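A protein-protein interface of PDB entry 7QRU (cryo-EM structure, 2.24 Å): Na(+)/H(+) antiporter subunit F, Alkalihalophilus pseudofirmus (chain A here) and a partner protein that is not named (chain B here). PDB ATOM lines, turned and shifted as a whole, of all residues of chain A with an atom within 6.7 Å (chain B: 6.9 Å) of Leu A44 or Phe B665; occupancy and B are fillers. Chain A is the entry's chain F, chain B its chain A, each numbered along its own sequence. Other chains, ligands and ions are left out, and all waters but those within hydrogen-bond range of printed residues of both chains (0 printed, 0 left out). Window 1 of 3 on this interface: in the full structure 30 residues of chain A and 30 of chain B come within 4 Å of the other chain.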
ATOM      1  N   MET A  13      24.205 -16.951  27.257  1.00  0.00           N
ATOM      2  CA  MET A  13      24.172 -18.237  26.588  1.00  0.00           C
ATOM      3  C   MET A  13      22.741 -18.806  26.472  1.00  0.00           C
ATOM      4  O   MET A  13      22.420 -19.550  25.532  1.00  0.00           O
ATOM      5  CB  MET A  13      24.995 -19.303  27.293  1.00  0.00           C
ATOM      6  CG  MET A  13      26.529 -19.066  27.441  1.00  0.00           C
ATOM      7  SD  MET A  13      27.235 -18.758  25.830  1.00  0.00           S
ATOM      8  CE  MET A  13      27.002 -20.289  24.892  1.00  0.00           C
ATOM      9  N   LEU A  17      20.625 -19.792  22.995  1.00  0.00           N
ATOM     10  CA  LEU A  17      19.884 -21.041  22.715  1.00  0.00           C
ATOM     11  C   LEU A  17      18.449 -20.732  22.271  1.00  0.00           C
ATOM     12  O   LEU A  17      17.972 -21.317  21.310  1.00  0.00           O
ATOM     13  CB  LEU A  17      19.853 -21.968  23.943  1.00  0.00           C
ATOM     14  CG  LEU A  17      21.215 -22.542  24.319  1.00  0.00           C
ATOM     15  CD1 LEU A  17      21.175 -23.148  25.697  1.00  0.00           C
ATOM     16  CD2 LEU A  17      21.698 -23.579  23.331  1.00  0.00           C
ATOM     17  N   LEU A  37      20.083 -26.162  14.402  1.00  0.00           N
ATOM     18  CA  LEU A  37      20.250 -27.268  15.340  1.00  0.00           C
ATOM     19  C   LEU A  37      21.739 -27.454  15.643  1.00  0.00           C
ATOM     20  O   LEU A  37      22.128 -27.711  16.773  1.00  0.00           O
ATOM     21  CB  LEU A  37      19.673 -28.570  14.764  1.00  0.00           C
ATOM     22  CG  LEU A  37      19.824 -29.808  15.663  1.00  0.00           C
ATOM     23  CD1 LEU A  37      19.114 -29.628  16.978  1.00  0.00           C
ATOM     24  CD2 LEU A  37      19.312 -31.071  15.011  1.00  0.00           C
ATOM     25  N   ASP A  38      22.571 -27.396  14.642  1.00  0.00           N
ATOM     26  CA  ASP A  38      23.991 -27.586  14.771  1.00  0.00           C
ATOM     27  C   ASP A  38      24.517 -26.479  15.684  1.00  0.00           C
ATOM     28  O   ASP A  38      25.362 -26.689  16.539  1.00  0.00           O
ATOM     29  CB  ASP A  38      24.677 -27.572  13.394  1.00  0.00           C
ATOM     30  CG  ASP A  38      26.179 -27.345  13.517  1.00  0.00           C
ATOM     31  OD1 ASP A  38      26.951 -28.343  13.915  1.00  0.00           O
ATOM     32  OD2 ASP A  38      26.571 -26.144  13.313  1.00  0.00           O
ATOM     33  N   THR A  39      24.090 -25.254  15.459  1.00  0.00           N
ATOM     34  CA  THR A  39      24.535 -24.156  16.319  1.00  0.00           C
ATOM     35  C   THR A  39      24.018 -24.277  17.775  1.00  0.00           C
ATOM     36  O   THR A  39      24.738 -23.994  18.727  1.00  0.00           O
ATOM     37  CB  THR A  39      24.083 -22.837  15.724  1.00  0.00           C
ATOM     38  OG1 THR A  39      24.323 -22.935  14.309  1.00  0.00           O
ATOM     39  CG2 THR A  39      24.744 -21.652  16.351  1.00  0.00           C
ATOM     40  N   PHE A  40      22.820 -24.834  17.980  1.00  0.00           N
ATOM     41  CA  PHE A  40      22.251 -25.040  19.299  1.00  0.00           C
ATOM     42  C   PHE A  40      23.187 -25.958  20.088  1.00  0.00           C
ATOM     43  O   PHE A  40      23.444 -25.748  21.278  1.00  0.00           O
ATOM     44  CB  PHE A  40      20.834 -25.632  19.130  1.00  0.00           C
ATOM     45  CG  PHE A  40      20.002 -25.673  20.397  1.00  0.00           C
ATOM     46  CD1 PHE A  40      20.086 -26.741  21.268  1.00  0.00           C
ATOM     47  CD2 PHE A  40      19.090 -24.680  20.682  1.00  0.00           C
ATOM     48  CE1 PHE A  40      19.317 -26.800  22.410  1.00  0.00           C
ATOM     49  CE2 PHE A  40      18.345 -24.706  21.845  1.00  0.00           C
ATOM     50  CZ  PHE A  40      18.470 -25.753  22.719  1.00  0.00           C
ATOM     51  N   GLY A  41      23.632 -27.067  19.462  1.00  0.00           N
ATOM     52  CA  GLY A  41      24.442 -28.034  20.150  1.00  0.00           C
ATOM     53  C   GLY A  41      25.826 -27.509  20.482  1.00  0.00           C
ATOM     54  O   GLY A  41      26.334 -27.732  21.585  1.00  0.00           O
ATOM     55  N   ILE A  42      26.444 -26.796  19.538  1.00  0.00           N
ATOM     56  CA  ILE A  42      27.736 -26.155  19.828  1.00  0.00           C
ATOM     57  C   ILE A  42      27.605 -25.215  21.025  1.00  0.00           C
ATOM     58  O   ILE A  42      28.490 -25.227  21.880  1.00  0.00           O
ATOM     59  CB  ILE A  42      28.275 -25.449  18.566  1.00  0.00           C
ATOM     60  CG1 ILE A  42      28.548 -26.523  17.486  1.00  0.00           C
ATOM     61  CG2 ILE A  42      29.478 -24.576  18.814  1.00  0.00           C
ATOM     62  CD1 ILE A  42      29.452 -27.651  18.003  1.00  0.00           C
ATOM     63  N   ASN A  43      26.541 -24.416  21.073  1.00  0.00           N
ATOM     64  CA  ASN A  43      26.339 -23.477  22.166  1.00  0.00           C
ATOM     65  C   ASN A  43      26.186 -24.172  23.518  1.00  0.00           C
ATOM     66  O   ASN A  43      26.614 -23.614  24.527  1.00  0.00           O
ATOM     67  CB  ASN A  43      25.156 -22.497  21.915  1.00  0.00           C
ATOM     68  CG  ASN A  43      25.503 -21.448  20.843  1.00  0.00           C
ATOM     69  OD1 ASN A  43      24.654 -20.852  20.189  1.00  0.00           O
ATOM     70  ND2 ASN A  43      26.763 -21.330  20.486  1.00  0.00           N
ATOM     71  N   LEU A  44      25.606 -25.379  23.544  1.00  0.00           N
ATOM     72  CA  LEU A  44      25.549 -26.161  24.762  1.00  0.00           C
ATOM     73  C   LEU A  44      26.913 -26.466  25.375  1.00  0.00           C
ATOM     74  O   LEU A  44      27.074 -26.405  26.575  1.00  0.00           O
ATOM     75  CB  LEU A  44      24.830 -27.468  24.482  1.00  0.00           C
ATOM     76  CG  LEU A  44      23.315 -27.433  24.340  1.00  0.00           C
ATOM     77  CD1 LEU A  44      22.899 -28.875  24.318  1.00  0.00           C
ATOM     78  CD2 LEU A  44      22.670 -26.671  25.462  1.00  0.00           C
ATOM     79  N   ILE A  45      27.937 -26.692  24.562  1.00  0.00           N
ATOM     80  CA  ILE A  45      29.296 -26.845  25.095  1.00  0.00           C
ATOM     81  C   ILE A  45      29.744 -25.612  25.871  1.00  0.00           C
ATOM     82  O   ILE A  45      30.282 -25.758  26.960  1.00  0.00           O
ATOM     83  CB  ILE A  45      30.317 -27.111  23.972  1.00  0.00           C
ATOM     84  CG1 ILE A  45      29.915 -28.319  23.149  1.00  0.00           C
ATOM     85  CG2 ILE A  45      31.720 -27.192  24.519  1.00  0.00           C
ATOM     86  CD1 ILE A  45      30.750 -28.389  21.957  1.00  0.00           C
ATOM     87  N   GLY A  46      29.439 -24.398  25.336  1.00  0.00           N
ATOM     88  CA  GLY A  46      29.746 -23.169  26.040  1.00  0.00           C
ATOM     89  C   GLY A  46      29.062 -23.168  27.407  1.00  0.00           C
ATOM     90  O   GLY A  46      29.642 -22.864  28.457  1.00  0.00           O
ATOM     91  N   PHE A  47      27.744 -23.411  27.370  1.00  0.00           N
ATOM     92  CA  PHE A  47      26.940 -23.371  28.570  1.00  0.00           C
ATOM     93  C   PHE A  47      27.490 -24.305  29.675  1.00  0.00           C
ATOM     94  O   PHE A  47      27.659 -23.887  30.826  1.00  0.00           O
ATOM     95  CB  PHE A  47      25.510 -23.760  28.194  1.00  0.00           C
ATOM     96  CG  PHE A  47      24.490 -23.323  29.188  1.00  0.00           C
ATOM     97  CD1 PHE A  47      24.287 -24.055  30.385  1.00  0.00           C
ATOM     98  CD2 PHE A  47      23.579 -22.337  28.810  1.00  0.00           C
ATOM     99  CE1 PHE A  47      23.296 -23.684  31.278  1.00  0.00           C
ATOM    100  CE2 PHE A  47      22.572 -21.987  29.684  1.00  0.00           C
ATOM    101  CZ  PHE A  47      22.429 -22.654  30.897  1.00  0.00           C
ATOM    102  N   ILE A  48      27.853 -25.521  29.318  1.00  0.00           N
ATOM    103  CA  ILE A  48      28.461 -26.452  30.255  1.00  0.00           C
ATOM    104  C   ILE A  48      29.858 -26.054  30.726  1.00  0.00           C
ATOM    105  O   ILE A  48      30.145 -26.133  31.924  1.00  0.00           O
ATOM    106  CB  ILE A  48      28.330 -27.865  29.663  1.00  0.00           C
ATOM    107  CG1 ILE A  48      26.817 -28.158  29.523  1.00  0.00           C
ATOM    108  CG2 ILE A  48      28.969 -28.946  30.553  1.00  0.00           C
ATOM    109  CD1 ILE A  48      26.575 -29.421  28.804  1.00  0.00           C
ATOM    110  N   GLY A  49      30.756 -25.618  29.859  1.00  0.00           N
ATOM    111  CA  GLY A  49      32.018 -25.081  30.329  1.00  0.00           C
ATOM    112  C   GLY A  49      31.783 -24.079  31.419  1.00  0.00           C
ATOM    113  O   GLY A  49      32.492 -24.098  32.392  1.00  0.00           O
ATOM    114  N   VAL A  64      31.184 -32.381  27.539  1.00  0.00           N
ATOM    115  CA  VAL A  64      31.371 -31.376  26.498  1.00  0.00           C
ATOM    116  C   VAL A  64      31.928 -32.097  25.296  1.00  0.00           C
ATOM    117  O   VAL A  64      31.526 -31.803  24.180  1.00  0.00           O
ATOM    118  CB  VAL A  64      32.206 -30.133  26.882  1.00  0.00           C
ATOM    119  CG1 VAL A  64      31.472 -29.263  27.900  1.00  0.00           C
ATOM    120  CG2 VAL A  64      33.496 -30.489  27.445  1.00  0.00           C
ATOM    121  N   ILE A  67      29.165 -33.884  23.433  1.00  0.00           N
ATOM    122  CA  ILE A  67      28.272 -33.029  22.681  1.00  0.00           C
ATOM    123  C   ILE A  67      28.953 -32.673  21.372  1.00  0.00           C
ATOM    124  O   ILE A  67      28.321 -32.615  20.345  1.00  0.00           O
ATOM    125  CB  ILE A  67      27.897 -31.753  23.454  1.00  0.00           C
ATOM    126  CG1 ILE A  67      26.980 -32.040  24.601  1.00  0.00           C
ATOM    127  CG2 ILE A  67      27.328 -30.698  22.518  1.00  0.00           C
ATOM    128  CD1 ILE A  67      26.980 -30.902  25.555  1.00  0.00           C
ATOM    129  N   LEU A  70      28.542 -35.616  19.060  1.00  0.00           N
ATOM    130  CA  LEU A  70      27.188 -35.896  18.609  1.00  0.00           C
ATOM    131  C   LEU A  70      26.604 -34.789  17.749  1.00  0.00           C
ATOM    132  O   LEU A  70      25.801 -35.106  16.876  1.00  0.00           O
ATOM    133  CB  LEU A  70      26.347 -36.167  19.881  1.00  0.00           C
ATOM    134  CG  LEU A  70      26.848 -37.491  20.572  1.00  0.00           C
ATOM    135  CD1 LEU A  70      26.041 -37.895  21.774  1.00  0.00           C
ATOM    136  CD2 LEU A  70      26.913 -38.733  19.618  1.00  0.00           C
ATOM    137  N   ALA A  71      26.865 -33.516  18.065  1.00  0.00           N
ATOM    138  CA  ALA A  71      26.332 -32.468  17.226  1.00  0.00           C
ATOM    139  C   ALA A  71      26.807 -32.677  15.777  1.00  0.00           C
ATOM    140  O   ALA A  71      26.042 -32.504  14.815  1.00  0.00           O
ATOM    141  CB  ALA A  71      26.711 -31.111  17.692  1.00  0.00           C
ATOM    142  N   ILE B 636      16.225 -21.397  29.991  1.00  0.00           N
ATOM    143  CA  ILE B 636      16.310 -22.769  29.490  1.00  0.00           C
ATOM    144  C   ILE B 636      14.923 -23.405  29.532  1.00  0.00           C
ATOM    145  O   ILE B 636      14.537 -24.105  28.639  1.00  0.00           O
ATOM    146  CB  ILE B 636      17.333 -23.586  30.330  1.00  0.00           C
ATOM    147  CG1 ILE B 636      18.754 -23.126  30.046  1.00  0.00           C
ATOM    148  CG2 ILE B 636      17.268 -25.057  30.081  1.00  0.00           C
ATOM    149  CD1 ILE B 636      18.998 -22.811  28.599  1.00  0.00           C
ATOM    150  N   PHE B 640      12.497 -25.059  26.655  1.00  0.00           N
ATOM    151  CA  PHE B 640      12.119 -26.453  26.717  1.00  0.00           C
ATOM    152  C   PHE B 640      10.601 -26.591  26.538  1.00  0.00           C
ATOM    153  O   PHE B 640      10.111 -27.453  25.786  1.00  0.00           O
ATOM    154  CB  PHE B 640      12.611 -27.002  28.047  1.00  0.00           C
ATOM    155  CG  PHE B 640      12.441 -28.477  28.161  1.00  0.00           C
ATOM    156  CD1 PHE B 640      11.243 -29.015  28.551  1.00  0.00           C
ATOM    157  CD2 PHE B 640      13.443 -29.334  27.759  1.00  0.00           C
ATOM    158  CE1 PHE B 640      11.071 -30.387  28.564  1.00  0.00           C
ATOM    159  CE2 PHE B 640      13.299 -30.705  27.850  1.00  0.00           C
ATOM    160  CZ  PHE B 640      12.098 -31.226  28.234  1.00  0.00           C
ATOM    161  N   VAL B 658      14.159 -32.488  14.168  1.00  0.00           N
ATOM    162  CA  VAL B 658      14.958 -31.410  14.710  1.00  0.00           C
ATOM    163  C   VAL B 658      14.465 -30.917  16.073  1.00  0.00           C
ATOM    164  O   VAL B 658      15.266 -30.743  16.966  1.00  0.00           O
ATOM    165  CB  VAL B 658      15.062 -30.244  13.716  1.00  0.00           C
ATOM    166  CG1 VAL B 658      15.692 -29.036  14.305  1.00  0.00           C
ATOM    167  CG2 VAL B 658      15.868 -30.690  12.489  1.00  0.00           C
ATOM    168  N   VAL B 660      12.572 -32.553  18.199  1.00  0.00           N
ATOM    169  CA  VAL B 660      12.851 -33.622  19.123  1.00  0.00           C
ATOM    170  C   VAL B 660      14.315 -33.637  19.592  1.00  0.00           C
ATOM    171  O   VAL B 660      14.549 -33.933  20.749  1.00  0.00           O
ATOM    172  CB  VAL B 660      12.362 -34.964  18.538  1.00  0.00           C
ATOM    173  CG1 VAL B 660      12.881 -36.157  19.283  1.00  0.00           C
ATOM    174  CG2 VAL B 660      10.852 -34.937  18.587  1.00  0.00           C
ATOM    175  N   GLY B 661      15.265 -33.489  18.707  1.00  0.00           N
ATOM    176  CA  GLY B 661      16.644 -33.199  19.051  1.00  0.00           C
ATOM    177  C   GLY B 661      16.805 -32.024  20.017  1.00  0.00           C
ATOM    178  O   GLY B 661      17.547 -32.084  20.992  1.00  0.00           O
ATOM    179  N   VAL B 662      16.215 -30.899  19.692  1.00  0.00           N
ATOM    180  CA  VAL B 662      16.320 -29.822  20.613  1.00  0.00           C
ATOM    181  C   VAL B 662      15.899 -30.333  21.981  1.00  0.00           C
ATOM    182  O   VAL B 662      16.533 -29.989  22.993  1.00  0.00           O
ATOM    183  CB  VAL B 662      15.549 -28.562  20.187  1.00  0.00           C
ATOM    184  CG1 VAL B 662      15.459 -27.583  21.343  1.00  0.00           C
ATOM    185  CG2 VAL B 662      16.230 -28.008  18.969  1.00  0.00           C
ATOM    186  N   ILE B 663      14.746 -30.968  22.053  1.00  0.00           N
ATOM    187  CA  ILE B 663      14.210 -31.373  23.352  1.00  0.00           C
ATOM    188  C   ILE B 663      15.188 -32.321  24.050  1.00  0.00           C
ATOM    189  O   ILE B 663      15.466 -32.180  25.259  1.00  0.00           O
ATOM    190  CB  ILE B 663      12.772 -31.955  23.218  1.00  0.00           C
ATOM    191  CG1 ILE B 663      11.778 -30.787  23.102  1.00  0.00           C
ATOM    192  CG2 ILE B 663      12.429 -32.796  24.404  1.00  0.00           C
ATOM    193  CD1 ILE B 663      10.576 -31.130  22.280  1.00  0.00           C
ATOM    194  N   GLY B 664      15.705 -33.277  23.301  1.00  0.00           N
ATOM    195  CA  GLY B 664      16.738 -34.181  23.776  1.00  0.00           C
ATOM    196  C   GLY B 664      18.007 -33.528  24.289  1.00  0.00           C
ATOM    197  O   GLY B 664      18.504 -33.887  25.323  1.00  0.00           O
ATOM    198  N   PHE B 665      18.540 -32.581  23.570  1.00  0.00           N
ATOM    199  CA  PHE B 665      19.666 -31.823  24.039  1.00  0.00           C
ATOM    200  C   PHE B 665      19.360 -31.034  25.300  1.00  0.00           C
ATOM    201  O   PHE B 665      20.248 -30.838  26.123  1.00  0.00           O
ATOM    202  CB  PHE B 665      20.060 -30.755  23.049  1.00  0.00           C
ATOM    203  CG  PHE B 665      21.019 -31.151  21.980  1.00  0.00           C
ATOM    204  CD1 PHE B 665      22.255 -31.702  22.298  1.00  0.00           C
ATOM    205  CD2 PHE B 665      20.763 -30.784  20.648  1.00  0.00           C
ATOM    206  CE1 PHE B 665      23.163 -31.988  21.277  1.00  0.00           C
ATOM    207  CE2 PHE B 665      21.639 -31.151  19.634  1.00  0.00           C
ATOM    208  CZ  PHE B 665      22.842 -31.733  19.954  1.00  0.00           C
ATOM    209  N   LEU B 666      18.199 -30.383  25.351  1.00  0.00           N
ATOM    210  CA  LEU B 666      17.856 -29.623  26.540  1.00  0.00           C
ATOM    211  C   LEU B 666      17.613 -30.523  27.758  1.00  0.00           C
ATOM    212  O   LEU B 666      17.971 -30.156  28.863  1.00  0.00           O
ATOM    213  CB  LEU B 666      16.650 -28.712  26.329  1.00  0.00           C
ATOM    214  CG  LEU B 666      16.974 -27.448  25.559  1.00  0.00           C
ATOM    215  CD1 LEU B 666      15.716 -26.665  25.240  1.00  0.00           C
ATOM    216  CD2 LEU B 666      18.007 -26.628  26.302  1.00  0.00           C
ATOM    217  N   LEU B 667      17.011 -31.667  27.601  1.00  0.00           N
ATOM    218  CA  LEU B 667      16.903 -32.577  28.733  1.00  0.00           C
ATOM    219  C   LEU B 667      18.319 -33.004  29.187  1.00  0.00           C
ATOM    220  O   LEU B 667      18.657 -32.896  30.353  1.00  0.00           O
ATOM    221  CB  LEU B 667      15.962 -33.714  28.317  1.00  0.00           C
ATOM    222  CG  LEU B 667      15.612 -34.641  29.441  1.00  0.00           C
ATOM    223  CD1 LEU B 667      14.775 -33.862  30.391  1.00  0.00           C
ATOM    224  CD2 LEU B 667      14.909 -35.930  28.962  1.00  0.00           C
ATOM    225  N   ALA B 668      19.271 -33.219  28.302  1.00  0.00           N
ATOM    226  CA  ALA B 668      20.640 -33.478  28.762  1.00  0.00           C
ATOM    227  C   ALA B 668      21.209 -32.297  29.508  1.00  0.00           C
ATOM    228  O   ALA B 668      21.836 -32.481  30.570  1.00  0.00           O
ATOM    229  CB  ALA B 668      21.542 -33.844  27.616  1.00  0.00           C
ATOM    230  N   LEU B 669      20.954 -31.079  29.041  1.00  0.00           N
ATOM    231  CA  LEU B 669      21.404 -29.895  29.781  1.00  0.00           C
ATOM    232  C   LEU B 669      20.799 -29.807  31.173  1.00  0.00           C
ATOM    233  O   LEU B 669      21.444 -29.438  32.151  1.00  0.00           O
ATOM    234  CB  LEU B 669      21.003 -28.680  28.944  1.00  0.00           C
ATOM    235  CG  LEU B 669      21.371 -27.335  29.576  1.00  0.00           C
ATOM    236  CD1 LEU B 669      22.828 -27.383  29.908  1.00  0.00           C
ATOM    237  CD2 LEU B 669      21.085 -26.149  28.680  1.00  0.00           C
ATOM    238  N   LEU B 670      19.504 -30.134  31.341  1.00  0.00           N
ATOM    239  CA  LEU B 670      18.936 -30.153  32.672  1.00  0.00           C
ATOM    240  C   LEU B 670      19.629 -31.201  33.525  1.00  0.00           C
ATOM    241  O   LEU B 670      19.841 -30.977  34.718  1.00  0.00           O
ATOM    242  CB  LEU B 670      17.431 -30.424  32.564  1.00  0.00           C
ATOM    243  CG  LEU B 670      16.607 -29.277  31.956  1.00  0.00           C
ATOM    244  CD1 LEU B 670      15.188 -29.728  31.873  1.00  0.00           C
ATOM    245  CD2 LEU B 670      16.668 -28.018  32.786  1.00  0.00           C
ATOM    246  N   GLN B 683      21.748 -39.751  27.989  1.00  0.00           N
ATOM    247  CA  GLN B 683      20.674 -39.097  27.306  1.00  0.00           C
ATOM    248  C   GLN B 683      21.148 -38.567  25.946  1.00  0.00           C
ATOM    249  O   GLN B 683      20.498 -38.784  24.951  1.00  0.00           O
ATOM    250  CB  GLN B 683      20.042 -38.034  28.180  1.00  0.00           C
ATOM    251  CG  GLN B 683      18.919 -37.268  27.469  1.00  0.00           C
ATOM    252  CD  GLN B 683      17.746 -38.190  27.272  1.00  0.00           C
ATOM    253  OE1 GLN B 683      17.435 -38.612  26.166  1.00  0.00           O
ATOM    254  NE2 GLN B 683      17.166 -38.612  28.390  1.00  0.00           N
ATOM    255  N   LEU B 684      22.336 -38.006  25.855  1.00  0.00           N
ATOM    256  CA  LEU B 684      22.858 -37.495  24.610  1.00  0.00           C
ATOM    257  C   LEU B 684      23.116 -38.580  23.593  1.00  0.00           C
ATOM    258  O   LEU B 684      22.802 -38.353  22.425  1.00  0.00           O
ATOM    259  CB  LEU B 684      24.170 -36.762  24.865  1.00  0.00           C
ATOM    260  CG  LEU B 684      24.041 -35.409  25.517  1.00  0.00           C
ATOM    261  CD1 LEU B 684      25.370 -34.944  25.989  1.00  0.00           C
ATOM    262  CD2 LEU B 684      23.457 -34.386  24.601  1.00  0.00           C
ATOM    263  N   GLU B 687      19.807 -39.998  22.395  1.00  0.00           N
ATOM    264  CA  GLU B 687      19.158 -39.064  21.487  1.00  0.00           C
ATOM    265  C   GLU B 687      19.782 -39.103  20.081  1.00  0.00           C
ATOM    266  O   GLU B 687      19.049 -39.118  19.078  1.00  0.00           O
ATOM    267  CB  GLU B 687      19.153 -37.666  22.107  1.00  0.00           C
ATOM    268  CG  GLU B 687      18.037 -37.509  23.145  1.00  0.00           C
ATOM    269  CD  GLU B 687      16.927 -38.562  23.060  1.00  0.00           C
ATOM    270  OE1 GLU B 687      17.079 -39.630  23.705  1.00  0.00           O
ATOM    271  OE2 GLU B 687      15.895 -38.334  22.343  1.00  0.00           O
ATOM    272  N   THR B 688      21.107 -39.255  19.991  1.00  0.00           N
ATOM    273  CA  THR B 688      21.773 -39.309  18.715  1.00  0.00           C
ATOM    274  C   THR B 688      21.369 -40.564  17.950  1.00  0.00           C
ATOM    275  O   THR B 688      21.102 -40.483  16.771  1.00  0.00           O
ATOM    276  CB  THR B 688      23.288 -39.075  18.908  1.00  0.00           C
ATOM    277  OG1 THR B 688      23.314 -37.648  19.099  1.00  0.00           O
ATOM    278  CG2 THR B 688      24.159 -39.544  17.767  1.00  0.00           C
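Printed residues of chain B within 4 Å of Leu A37: Val B662 (3.9 Å) and Phe B665 (3.97 Å).
Printed residues of chain B within 4 Å of Phe A47: Ile B636 (3.8 Å) and Leu B669 (3.7 Å).
Of the printed residues of chain A, Val B662 touches Leu A37 (3.9 Å) and Phe A40 (3.8 Å).
Of chain A, only Leu A37 and Leu A44 come within 4 Å of Phe B665.
Leu B667 touches none of the printed residues of chain A.
Printed residues of chain A within 4 Å of Leu B684: Ile A67 (3.6 Å) and Leu A70 (3.3 Å).
Of the printed residues of chain A, Thr B688 touches Leu A70 (3.4 Å).
The nearest residue of chain B that does not touch Leu A44 is Leu B666 (4.7 Å).
The nearest printed residue of chain B that does not touch Phe A47 is Leu B666 (7.3 Å).
Of the 18 printed residues of chain B, 7 touch a printed residue of chain A.
Hydrophobic or aromatic side chains of chain B within 4 Å of the printed part of chain A: Ile B636, Val B662, Phe B665, Leu B666, Leu B669 and Leu B684.
Along chain B the printed residues that touch a printed residue of chain A span positions 636 to 688.
Hydrophobic or aromatic side chains of chain A within 4 Å of the printed part of chain B: Leu A17, Leu A37, Phe A40, Leu A44, Phe A47, Ile A67 and Leu A70.
Among the printed residues, 12 pairs touch across the chains.
Among the printed residues, no Asp or Glu carboxylate lies within 4 Å of a Lys or Arg side-chain nitrogen of the other chain.
Among the printed residues, pairs that only touch across the chains: Leu A70 with Leu B684, Leu A70 with Thr B688, Leu A44 with Phe B665, Ile A67 with Leu B684, Leu A44 with Leu B669, Phe A40 with Leu B666, Leu A17 with Ile B636, Phe A47 with Leu B669, Phe A40 with Val B662, Phe A47 with Ile B636, Leu A37 with Val B662 and Leu A37 with Phe B665.
The backbone carbonyl oxygen (O) of Leu B684 lies within hydrogen-bond range of the side-chain hydroxyl (OG1) of Thr B688, at 3.4 Å.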
